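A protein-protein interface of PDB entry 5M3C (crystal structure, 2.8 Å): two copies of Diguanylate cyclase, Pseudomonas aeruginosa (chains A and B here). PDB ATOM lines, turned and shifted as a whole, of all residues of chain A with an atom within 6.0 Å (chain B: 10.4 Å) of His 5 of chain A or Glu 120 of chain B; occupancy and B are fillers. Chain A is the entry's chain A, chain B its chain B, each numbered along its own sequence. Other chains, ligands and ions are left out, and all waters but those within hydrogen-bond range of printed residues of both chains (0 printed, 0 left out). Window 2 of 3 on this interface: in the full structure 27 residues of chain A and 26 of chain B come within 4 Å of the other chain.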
ATOM      1  N   HIS A   4       1.805 -14.561  -4.778  1.00  0.00           N
ATOM      2  CA  HIS A   4       1.827 -14.882  -3.319  1.00  0.00           C
ATOM      3  C   HIS A   4       3.235 -14.729  -2.728  1.00  0.00           C
ATOM      4  O   HIS A   4       3.402 -14.670  -1.508  1.00  0.00           O
ATOM      5  CB  HIS A   4       1.293 -16.303  -3.084  1.00  0.00           C
ATOM      6  CG  HIS A   4       0.393 -16.423  -1.889  1.00  0.00           C
ATOM      7  ND1 HIS A   4      -0.585 -15.496  -1.597  1.00  0.00           N
ATOM      8  CD2 HIS A   4       0.304 -17.377  -0.932  1.00  0.00           C
ATOM      9  CE1 HIS A   4      -1.225 -15.864  -0.502  1.00  0.00           C
ATOM     10  NE2 HIS A   4      -0.707 -17.003  -0.080  1.00  0.00           N
ATOM     11  N   HIS A   5       4.240 -14.667  -3.598  1.00  0.00           N
ATOM     12  CA  HIS A   5       5.623 -14.443  -3.182  1.00  0.00           C
ATOM     13  C   HIS A   5       6.190 -13.200  -3.867  1.00  0.00           C
ATOM     14  O   HIS A   5       5.848 -12.901  -5.011  1.00  0.00           O
ATOM     15  CB  HIS A   5       6.490 -15.657  -3.533  1.00  0.00           C
ATOM     16  CG  HIS A   5       6.170 -16.883  -2.738  1.00  0.00           C
ATOM     17  ND1 HIS A   5       5.049 -17.652  -2.970  1.00  0.00           N
ATOM     18  CD2 HIS A   5       6.829 -17.481  -1.717  1.00  0.00           C
ATOM     19  CE1 HIS A   5       5.028 -18.666  -2.122  1.00  0.00           C
ATOM     20  NE2 HIS A   5       6.098 -18.584  -1.352  1.00  0.00           N
ATOM     21  N   ASP A   6       7.058 -12.479  -3.163  1.00  0.00           N
ATOM     22  CA  ASP A   6       7.723 -11.313  -3.737  1.00  0.00           C
ATOM     23  C   ASP A   6       8.600 -11.734  -4.910  1.00  0.00           C
ATOM     24  O   ASP A   6       9.536 -12.513  -4.739  1.00  0.00           O
ATOM     25  CB  ASP A   6       8.574 -10.596  -2.682  1.00  0.00           C
ATOM     26  CG  ASP A   6       9.593  -9.647  -3.298  1.00  0.00           C
ATOM     27  OD1 ASP A   6      10.583 -10.132  -3.883  1.00  0.00           O
ATOM     28  OD2 ASP A   6       9.410  -8.417  -3.191  1.00  0.00           O
ATOM     29  N   PRO A   7       8.304 -11.208  -6.107  1.00  0.00           N
ATOM     30  CA  PRO A   7       9.045 -11.576  -7.313  1.00  0.00           C
ATOM     31  C   PRO A   7      10.547 -11.345  -7.184  1.00  0.00           C
ATOM     32  O   PRO A   7      11.336 -12.239  -7.481  1.00  0.00           O
ATOM     33  CB  PRO A   7       8.458 -10.654  -8.392  1.00  0.00           C
ATOM     34  CG  PRO A   7       7.748  -9.567  -7.655  1.00  0.00           C
ATOM     35  CD  PRO A   7       7.273 -10.192  -6.382  1.00  0.00           C
ATOM     36  N   GLY A  10      11.723 -13.552  -4.105  1.00  0.00           N
ATOM     37  CA  GLY A  10      11.098 -14.871  -4.028  1.00  0.00           C
ATOM     38  C   GLY A  10      10.589 -15.207  -2.637  1.00  0.00           C
ATOM     39  O   GLY A  10      10.114 -16.318  -2.392  1.00  0.00           O
ATOM     40  N   LEU A  11      10.679 -14.241  -1.727  1.00  0.00           N
ATOM     41  CA  LEU A  11      10.267 -14.446  -0.345  1.00  0.00           C
ATOM     42  C   LEU A  11       8.766 -14.278  -0.193  1.00  0.00           C
ATOM     43  O   LEU A  11       8.147 -13.537  -0.953  1.00  0.00           O
ATOM     44  CB  LEU A  11      10.974 -13.449   0.566  1.00  0.00           C
ATOM     45  CG  LEU A  11      12.481 -13.640   0.700  1.00  0.00           C
ATOM     46  CD1 LEU A  11      13.114 -12.405   1.321  1.00  0.00           C
ATOM     47  CD2 LEU A  11      12.787 -14.877   1.526  1.00  0.00           C
ATOM     48  N   PRO A  12       8.174 -14.967   0.796  1.00  0.00           N
ATOM     49  CA  PRO A  12       6.755 -14.834   1.105  1.00  0.00           C
ATOM     50  C   PRO A  12       6.333 -13.381   1.252  1.00  0.00           C
ATOM     51  O   PRO A  12       7.129 -12.541   1.675  1.00  0.00           O
ATOM     52  CB  PRO A  12       6.622 -15.551   2.448  1.00  0.00           C
ATOM     53  CG  PRO A  12       7.700 -16.574   2.433  1.00  0.00           C
ATOM     54  CD  PRO A  12       8.835 -15.967   1.654  1.00  0.00           C
ATOM     55  N   ASN A  13       5.084 -13.093   0.908  1.00  0.00           N
ATOM     56  CA  ASN A  13       4.554 -11.741   1.026  1.00  0.00           C
ATOM     57  C   ASN A  13       3.957 -11.513   2.411  1.00  0.00           C
ATOM     58  O   ASN A  13       3.798 -12.451   3.199  1.00  0.00           O
ATOM     59  CB  ASN A  13       3.495 -11.484  -0.051  1.00  0.00           C
ATOM     60  CG  ASN A  13       2.314 -12.434   0.047  1.00  0.00           C
ATOM     61  OD1 ASN A  13       2.052 -13.016   1.101  1.00  0.00           O
ATOM     62  ND2 ASN A  13       1.591 -12.598  -1.058  1.00  0.00           N
ATOM     63  N   LEU A  16       0.933 -14.037   3.165  1.00  0.00           N
ATOM     64  CA  LEU A  16       1.367 -15.391   3.508  1.00  0.00           C
ATOM     65  C   LEU A  16       1.947 -15.441   4.919  1.00  0.00           C
ATOM     66  O   LEU A  16       1.529 -16.258   5.745  1.00  0.00           O
ATOM     67  CB  LEU A  16       2.401 -15.895   2.497  1.00  0.00           C
ATOM     68  CG  LEU A  16       2.915 -17.323   2.702  1.00  0.00           C
ATOM     69  CD1 LEU A  16       1.774 -18.325   2.812  1.00  0.00           C
ATOM     70  CD2 LEU A  16       3.852 -17.717   1.569  1.00  0.00           C
ATOM     71  N   ARG A  20       1.026 -17.759   8.305  1.00  0.00           N
ATOM     72  CA  ARG A  20       1.951 -18.602   9.053  1.00  0.00           C
ATOM     73  C   ARG A  20       1.924 -18.216  10.524  1.00  0.00           C
ATOM     74  O   ARG A  20       1.854 -19.072  11.407  1.00  0.00           O
ATOM     75  CB  ARG A  20       3.375 -18.425   8.528  1.00  0.00           C
ATOM     76  CG  ARG A  20       3.513 -18.453   7.015  1.00  0.00           C
ATOM     77  CD  ARG A  20       4.000 -19.798   6.504  1.00  0.00           C
ATOM     78  NE  ARG A  20       4.900 -19.626   5.367  1.00  0.00           N
ATOM     79  CZ  ARG A  20       5.363 -20.616   4.611  1.00  0.00           C
ATOM     80  NH1 ARG A  20       5.008 -21.872   4.855  1.00  0.00           N
ATOM     81  NH2 ARG A  20       6.180 -20.345   3.602  1.00  0.00           N
ATOM     82  N   ILE B  48      20.608 -30.454   1.013  1.00  0.00           N
ATOM     83  CA  ILE B  48      19.158 -30.562   0.934  1.00  0.00           C
ATOM     84  C   ILE B  48      18.697 -31.988   1.241  1.00  0.00           C
ATOM     85  O   ILE B  48      17.791 -32.195   2.054  1.00  0.00           O
ATOM     86  CB  ILE B  48      18.645 -30.111  -0.449  1.00  0.00           C
ATOM     87  CG1 ILE B  48      18.749 -28.588  -0.560  1.00  0.00           C
ATOM     88  CG2 ILE B  48      17.211 -30.567  -0.672  1.00  0.00           C
ATOM     89  CD1 ILE B  48      18.259 -28.029  -1.876  1.00  0.00           C
ATOM     90  N   LEU B  52      16.570 -32.844   4.511  1.00  0.00           N
ATOM     91  CA  LEU B  52      15.152 -33.113   4.231  1.00  0.00           C
ATOM     92  C   LEU B  52      14.865 -34.552   3.798  1.00  0.00           C
ATOM     93  O   LEU B  52      13.760 -35.054   4.006  1.00  0.00           O
ATOM     94  CB  LEU B  52      14.631 -32.161   3.155  1.00  0.00           C
ATOM     95  CG  LEU B  52      14.972 -30.684   3.331  1.00  0.00           C
ATOM     96  CD1 LEU B  52      14.326 -29.878   2.217  1.00  0.00           C
ATOM     97  CD2 LEU B  52      14.530 -30.176   4.694  1.00  0.00           C
ATOM     98  N   ILE B  56      11.739 -35.751  -0.331  1.00  0.00           N
ATOM     99  CA  ILE B  56      11.550 -34.316  -0.555  1.00  0.00           C
ATOM    100  C   ILE B  56      12.408 -33.827  -1.723  1.00  0.00           C
ATOM    101  O   ILE B  56      11.932 -33.093  -2.597  1.00  0.00           O
ATOM    102  CB  ILE B  56      11.903 -33.501   0.705  1.00  0.00           C
ATOM    103  N   LEU B  59      10.928 -34.606  -5.121  1.00  0.00           N
ATOM    104  CA  LEU B  59       9.877 -33.632  -5.396  1.00  0.00           C
ATOM    105  C   LEU B  59      10.498 -32.297  -5.807  1.00  0.00           C
ATOM    106  O   LEU B  59      10.012 -31.629  -6.723  1.00  0.00           O
ATOM    107  CB  LEU B  59       8.983 -33.449  -4.165  1.00  0.00           C
ATOM    108  N   LEU B  60      11.579 -31.917  -5.130  1.00  0.00           N
ATOM    109  CA  LEU B  60      12.298 -30.695  -5.479  1.00  0.00           C
ATOM    110  C   LEU B  60      12.870 -30.756  -6.893  1.00  0.00           C
ATOM    111  O   LEU B  60      12.756 -29.796  -7.653  1.00  0.00           O
ATOM    112  CB  LEU B  60      13.417 -30.416  -4.476  1.00  0.00           C
ATOM    113  CG  LEU B  60      12.969 -29.850  -3.128  1.00  0.00           C
ATOM    114  CD1 LEU B  60      14.171 -29.611  -2.229  1.00  0.00           C
ATOM    115  CD2 LEU B  60      12.178 -28.564  -3.316  1.00  0.00           C
ATOM    116  N   ALA B  63      10.103 -30.567  -9.322  1.00  0.00           N
ATOM    117  CA  ALA B  63       9.618 -29.187  -9.335  1.00  0.00           C
ATOM    118  C   ALA B  63      10.547 -28.274 -10.127  1.00  0.00           C
ATOM    119  O   ALA B  63      10.091 -27.431 -10.901  1.00  0.00           O
ATOM    120  CB  ALA B  63       9.468 -28.673  -7.912  1.00  0.00           C
ATOM    121  N   ARG B  67       9.746 -26.254 -13.785  1.00  0.00           N
ATOM    122  CA  ARG B  67       9.819 -24.794 -13.844  1.00  0.00           C
ATOM    123  C   ARG B  67      10.767 -24.303 -14.937  1.00  0.00           C
ATOM    124  O   ARG B  67      10.540 -23.250 -15.529  1.00  0.00           O
ATOM    125  CB  ARG B  67      10.240 -24.203 -12.500  1.00  0.00           C
ATOM    126  CG  ARG B  67      10.162 -22.684 -12.474  1.00  0.00           C
ATOM    127  CD  ARG B  67      10.523 -22.116 -11.115  1.00  0.00           C
ATOM    128  NE  ARG B  67       9.576 -22.525 -10.085  1.00  0.00           N
ATOM    129  CZ  ARG B  67       9.661 -22.166  -8.810  1.00  0.00           C
ATOM    130  NH1 ARG B  67      10.654 -21.382  -8.403  1.00  0.00           N
ATOM    131  NH2 ARG B  67       8.750 -22.591  -7.940  1.00  0.00           N
ATOM    132  N   PHE B 110      15.221 -19.731 -10.247  1.00  0.00           N
ATOM    133  CA  PHE B 110      15.614 -20.260  -8.943  1.00  0.00           C
ATOM    134  C   PHE B 110      15.445 -19.233  -7.823  1.00  0.00           C
ATOM    135  O   PHE B 110      15.703 -19.533  -6.655  1.00  0.00           O
ATOM    136  CB  PHE B 110      17.068 -20.739  -8.982  1.00  0.00           C
ATOM    137  CG  PHE B 110      17.269 -21.992  -9.784  1.00  0.00           C
ATOM    138  CD1 PHE B 110      17.064 -23.237  -9.211  1.00  0.00           C
ATOM    139  CD2 PHE B 110      17.654 -21.927 -11.112  1.00  0.00           C
ATOM    140  CE1 PHE B 110      17.242 -24.393  -9.945  1.00  0.00           C
ATOM    141  CE2 PHE B 110      17.836 -23.080 -11.852  1.00  0.00           C
ATOM    142  CZ  PHE B 110      17.630 -24.315 -11.267  1.00  0.00           C
ATOM    143  N   THR B 111      15.018 -18.025  -8.178  1.00  0.00           N
ATOM    144  CA  THR B 111      14.806 -16.971  -7.192  1.00  0.00           C
ATOM    145  C   THR B 111      13.686 -17.357  -6.235  1.00  0.00           C
ATOM    146  O   THR B 111      13.856 -17.331  -5.018  1.00  0.00           O
ATOM    147  CB  THR B 111      14.459 -15.634  -7.866  1.00  0.00           C
ATOM    148  OG1 THR B 111      15.649 -15.059  -8.419  1.00  0.00           O
ATOM    149  N   ALA B 112      12.538 -17.723  -6.792  1.00  0.00           N
ATOM    150  CA  ALA B 112      11.420 -18.190  -5.982  1.00  0.00           C
ATOM    151  C   ALA B 112      11.718 -19.580  -5.427  1.00  0.00           C
ATOM    152  O   ALA B 112      12.468 -20.349  -6.030  1.00  0.00           O
ATOM    153  CB  ALA B 112      10.143 -18.214  -6.808  1.00  0.00           C
ATOM    154  N   PRO B 113      11.122 -19.913  -4.274  1.00  0.00           N
ATOM    155  CA  PRO B 113      11.328 -21.237  -3.713  1.00  0.00           C
ATOM    156  C   PRO B 113      10.522 -22.271  -4.481  1.00  0.00           C
ATOM    157  O   PRO B 113       9.750 -21.914  -5.371  1.00  0.00           O
ATOM    158  CB  PRO B 113      10.809 -21.098  -2.280  1.00  0.00           C
ATOM    159  CG  PRO B 113       9.807 -19.992  -2.332  1.00  0.00           C
ATOM    160  CD  PRO B 113      10.098 -19.147  -3.542  1.00  0.00           C
ATOM    161  N   PHE B 114      10.703 -23.542  -4.142  1.00  0.00           N
ATOM    162  CA  PHE B 114       9.998 -24.618  -4.822  1.00  0.00           C
ATOM    163  C   PHE B 114       9.129 -25.376  -3.829  1.00  0.00           C
ATOM    164  O   PHE B 114       9.503 -25.546  -2.670  1.00  0.00           O
ATOM    165  CB  PHE B 114      10.992 -25.554  -5.508  1.00  0.00           C
ATOM    166  CG  PHE B 114      11.833 -24.877  -6.555  1.00  0.00           C
ATOM    167  CD1 PHE B 114      12.929 -24.109  -6.192  1.00  0.00           C
ATOM    168  CD2 PHE B 114      11.527 -25.004  -7.902  1.00  0.00           C
ATOM    169  CE1 PHE B 114      13.704 -23.483  -7.152  1.00  0.00           C
ATOM    170  CE2 PHE B 114      12.299 -24.380  -8.866  1.00  0.00           C
ATOM    171  CZ  PHE B 114      13.390 -23.619  -8.490  1.00  0.00           C
ATOM    172  N   GLN B 115       7.972 -25.834  -4.291  1.00  0.00           N
ATOM    173  CA  GLN B 115       6.966 -26.396  -3.400  1.00  0.00           C
ATOM    174  C   GLN B 115       7.067 -27.917  -3.286  1.00  0.00           C
ATOM    175  O   GLN B 115       6.873 -28.638  -4.267  1.00  0.00           O
ATOM    176  CB  GLN B 115       5.566 -26.004  -3.882  1.00  0.00           C
ATOM    177  CG  GLN B 115       4.571 -25.766  -2.756  1.00  0.00           C
ATOM    178  CD  GLN B 115       4.744 -24.406  -2.098  1.00  0.00           C
ATOM    179  OE1 GLN B 115       5.105 -23.427  -2.755  1.00  0.00           O
ATOM    180  NE2 GLN B 115       4.478 -24.338  -0.798  1.00  0.00           N
ATOM    181  N   ALA B 116       7.373 -28.390  -2.079  1.00  0.00           N
ATOM    182  CA  ALA B 116       7.388 -29.822  -1.775  1.00  0.00           C
ATOM    183  C   ALA B 116       6.560 -30.074  -0.517  1.00  0.00           C
ATOM    184  O   ALA B 116       6.770 -29.427   0.507  1.00  0.00           O
ATOM    185  CB  ALA B 116       8.814 -30.314  -1.586  1.00  0.00           C
ATOM    186  N   ASP B 117       5.639 -31.032  -0.605  1.00  0.00           N
ATOM    187  CA  ASP B 117       4.559 -31.199   0.382  1.00  0.00           C
ATOM    188  C   ASP B 117       4.053 -29.846   0.903  1.00  0.00           C
ATOM    189  O   ASP B 117       3.675 -28.980   0.111  1.00  0.00           O
ATOM    190  CB  ASP B 117       4.943 -32.164   1.525  1.00  0.00           C
ATOM    191  CG  ASP B 117       6.386 -32.017   1.976  1.00  0.00           C
ATOM    192  OD1 ASP B 117       6.738 -30.966   2.555  1.00  0.00           O
ATOM    193  OD2 ASP B 117       7.164 -32.974   1.773  1.00  0.00           O
ATOM    194  N   GLY B 118       4.039 -29.663   2.219  1.00  0.00           N
ATOM    195  CA  GLY B 118       3.480 -28.450   2.809  1.00  0.00           C
ATOM    196  C   GLY B 118       4.354 -27.229   2.611  1.00  0.00           C
ATOM    197  O   GLY B 118       3.854 -26.112   2.478  1.00  0.00           O
ATOM    198  N   HIS B 119       5.663 -27.445   2.574  1.00  0.00           N
ATOM    199  CA  HIS B 119       6.617 -26.345   2.632  1.00  0.00           C
ATOM    200  C   HIS B 119       7.130 -25.903   1.281  1.00  0.00           C
ATOM    201  O   HIS B 119       6.720 -26.400   0.229  1.00  0.00           O
ATOM    202  CB  HIS B 119       7.813 -26.745   3.488  1.00  0.00           C
ATOM    203  CG  HIS B 119       7.430 -27.318   4.810  1.00  0.00           C
ATOM    204  ND1 HIS B 119       7.812 -26.751   6.006  1.00  0.00           N
ATOM    205  CD2 HIS B 119       6.675 -28.396   5.124  1.00  0.00           C
ATOM    206  CE1 HIS B 119       7.318 -27.465   7.002  1.00  0.00           C
ATOM    207  NE2 HIS B 119       6.624 -28.468   6.493  1.00  0.00           N
ATOM    208  N   GLU B 120       8.048 -24.951   1.344  1.00  0.00           N
ATOM    209  CA  GLU B 120       8.717 -24.441   0.176  1.00  0.00           C
ATOM    210  C   GLU B 120      10.163 -24.182   0.567  1.00  0.00           C
ATOM    211  O   GLU B 120      10.440 -23.535   1.581  1.00  0.00           O
ATOM    212  CB  GLU B 120       8.051 -23.151  -0.287  1.00  0.00           C
ATOM    213  CG  GLU B 120       8.609 -21.906   0.380  1.00  0.00           C
ATOM    214  CD  GLU B 120       7.653 -20.737   0.329  1.00  0.00           C
ATOM    215  OE1 GLU B 120       6.651 -20.819  -0.415  1.00  0.00           O
ATOM    216  OE2 GLU B 120       7.905 -19.737   1.035  1.00  0.00           O
ATOM    217  N   PHE B 121      11.084 -24.703  -0.231  1.00  0.00           N
ATOM    218  CA  PHE B 121      12.498 -24.535   0.035  1.00  0.00           C
ATOM    219  C   PHE B 121      13.164 -23.861  -1.154  1.00  0.00           C
ATOM    220  O   PHE B 121      12.750 -24.054  -2.300  1.00  0.00           O
ATOM    221  CB  PHE B 121      13.135 -25.894   0.301  1.00  0.00           C
ATOM    222  CG  PHE B 121      12.377 -26.728   1.289  1.00  0.00           C
ATOM    223  CD1 PHE B 121      11.323 -27.526   0.876  1.00  0.00           C
ATOM    224  CD2 PHE B 121      12.714 -26.710   2.631  1.00  0.00           C
ATOM    225  CE1 PHE B 121      10.621 -28.295   1.784  1.00  0.00           C
ATOM    226  CE2 PHE B 121      12.017 -27.476   3.545  1.00  0.00           C
ATOM    227  CZ  PHE B 121      10.969 -28.270   3.121  1.00  0.00           C
ATOM    228  N   PHE B 122      14.192 -23.067  -0.879  1.00  0.00           N
ATOM    229  CA  PHE B 122      14.929 -22.394  -1.937  1.00  0.00           C
ATOM    230  C   PHE B 122      16.154 -23.204  -2.325  1.00  0.00           C
ATOM    231  O   PHE B 122      16.981 -23.550  -1.481  1.00  0.00           O
ATOM    232  CB  PHE B 122      15.371 -21.000  -1.499  1.00  0.00           C
ATOM    233  CG  PHE B 122      14.241 -20.109  -1.077  1.00  0.00           C
ATOM    234  CD1 PHE B 122      13.691 -20.225   0.189  1.00  0.00           C
ATOM    235  CD2 PHE B 122      13.732 -19.152  -1.942  1.00  0.00           C
ATOM    236  CE1 PHE B 122      12.652 -19.408   0.585  1.00  0.00           C
ATOM    237  CE2 PHE B 122      12.691 -18.331  -1.551  1.00  0.00           C
ATOM    238  CZ  PHE B 122      12.151 -18.460  -0.285  1.00  0.00           C
ATOM    239  N   VAL B 123      16.262 -23.502  -3.614  1.00  0.00           N
ATOM    240  CA  VAL B 123      17.439 -24.164  -4.150  1.00  0.00           C
ATOM    241  C   VAL B 123      18.051 -23.259  -5.211  1.00  0.00           C
ATOM    242  O   VAL B 123      17.349 -22.476  -5.852  1.00  0.00           O
ATOM    243  CB  VAL B 123      17.099 -25.538  -4.764  1.00  0.00           C
ATOM    244  CG1 VAL B 123      16.128 -26.297  -3.872  1.00  0.00           C
ATOM    245  CG2 VAL B 123      16.513 -25.372  -6.154  1.00  0.00           C
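A ring nitrogen (NE2) of His 5 of chain A is in hydrogen-bond range of the side-chain carboxylate (OE1) of Glu 120 of chain B.
OE2 of Glu 120 of chain B is in salt-bridge range of NH2 of Arg 20 of chain A, 3.2 Å away.
NH1 of Arg 67 of chain B lies within hydrogen-bond range of O of Ala 112 of chain B.
NH2 of Arg 67 of chain B sits at hydrogen-bond distance from O of Pro 113 of chain B, 2.8 Å away.
Among the printed residues, pairs that only touch across the chains: Gly 10 of chain A with Pro 113 of chain B (3.1 Å), Gly 10 of chain A with Phe 122 of chain B (3.4 Å), Pro 12 of chain A with Glu 120 of chain B (3.5 Å), Gly 10 of chain A with Thr 111 of chain B (3.8 Å), Gly 10 of chain A with Ala 112 of chain B (3.9 Å) and His 5 of chain A with Pro 113 of chain B (3.9 Å).
Of chain B, only Pro 113 (3.9 Å) and Glu 120 (2.5 Å) come within 4 Å of His 5 of chain A.
Asp 6 of chain A touches none of the printed residues of chain B.
Of chain B, only Thr 111 (3.8 Å), Ala 112 (3.9 Å), Pro 113 (3.1 Å) and Phe 122 (3.4 Å) come within 4 Å of Gly 10 of chain A.
Of chain B, only Glu 120 (3.5 Å) comes within 4 Å of Pro 12 of chain A.
Leu 16 of chain A touches none of the printed residues of chain B.
Of the printed residues of chain B, Arg 20 of chain A touches Glu 120.
Of the printed residues of chain A, Thr 111 of chain B touches Gly 10 (3.8 Å).
Printed residues of chain A within 4 Å of Ala 112 of chain B: Gly 10 (3.9 Å).
Printed residues of chain A within 4 Å of Pro 113 of chain B: His 5 and Gly 10.
His 119 of chain B touches none of the printed residues of chain A.
Of chain A, only His 5, Pro 12 and Arg 20 come within 4 Å of Glu 120 of chain B.
Of the printed residues of chain A, Phe 122 of chain B touches Gly 10 (3.4 Å).
The nearest printed residue of chain A that does not touch Ala 112 of chain B is His 5 of chain A (5.5 Å).
Hydrophobic or aromatic side chains of chain A within 4 Å of the printed part of chain B: His 5 and Pro 12.
Of the 21 printed residues of chain B, 5 touch a printed residue of chain A.
Hydrophobic or aromatic side chains of chain B within 4 Å of the printed part of chain A: Pro 113 and Phe 122.
No position is printed for both chains.
Of the 8 pairs that touch across the chains among the printed residues, none has its exchanged pair printed and touching as well.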
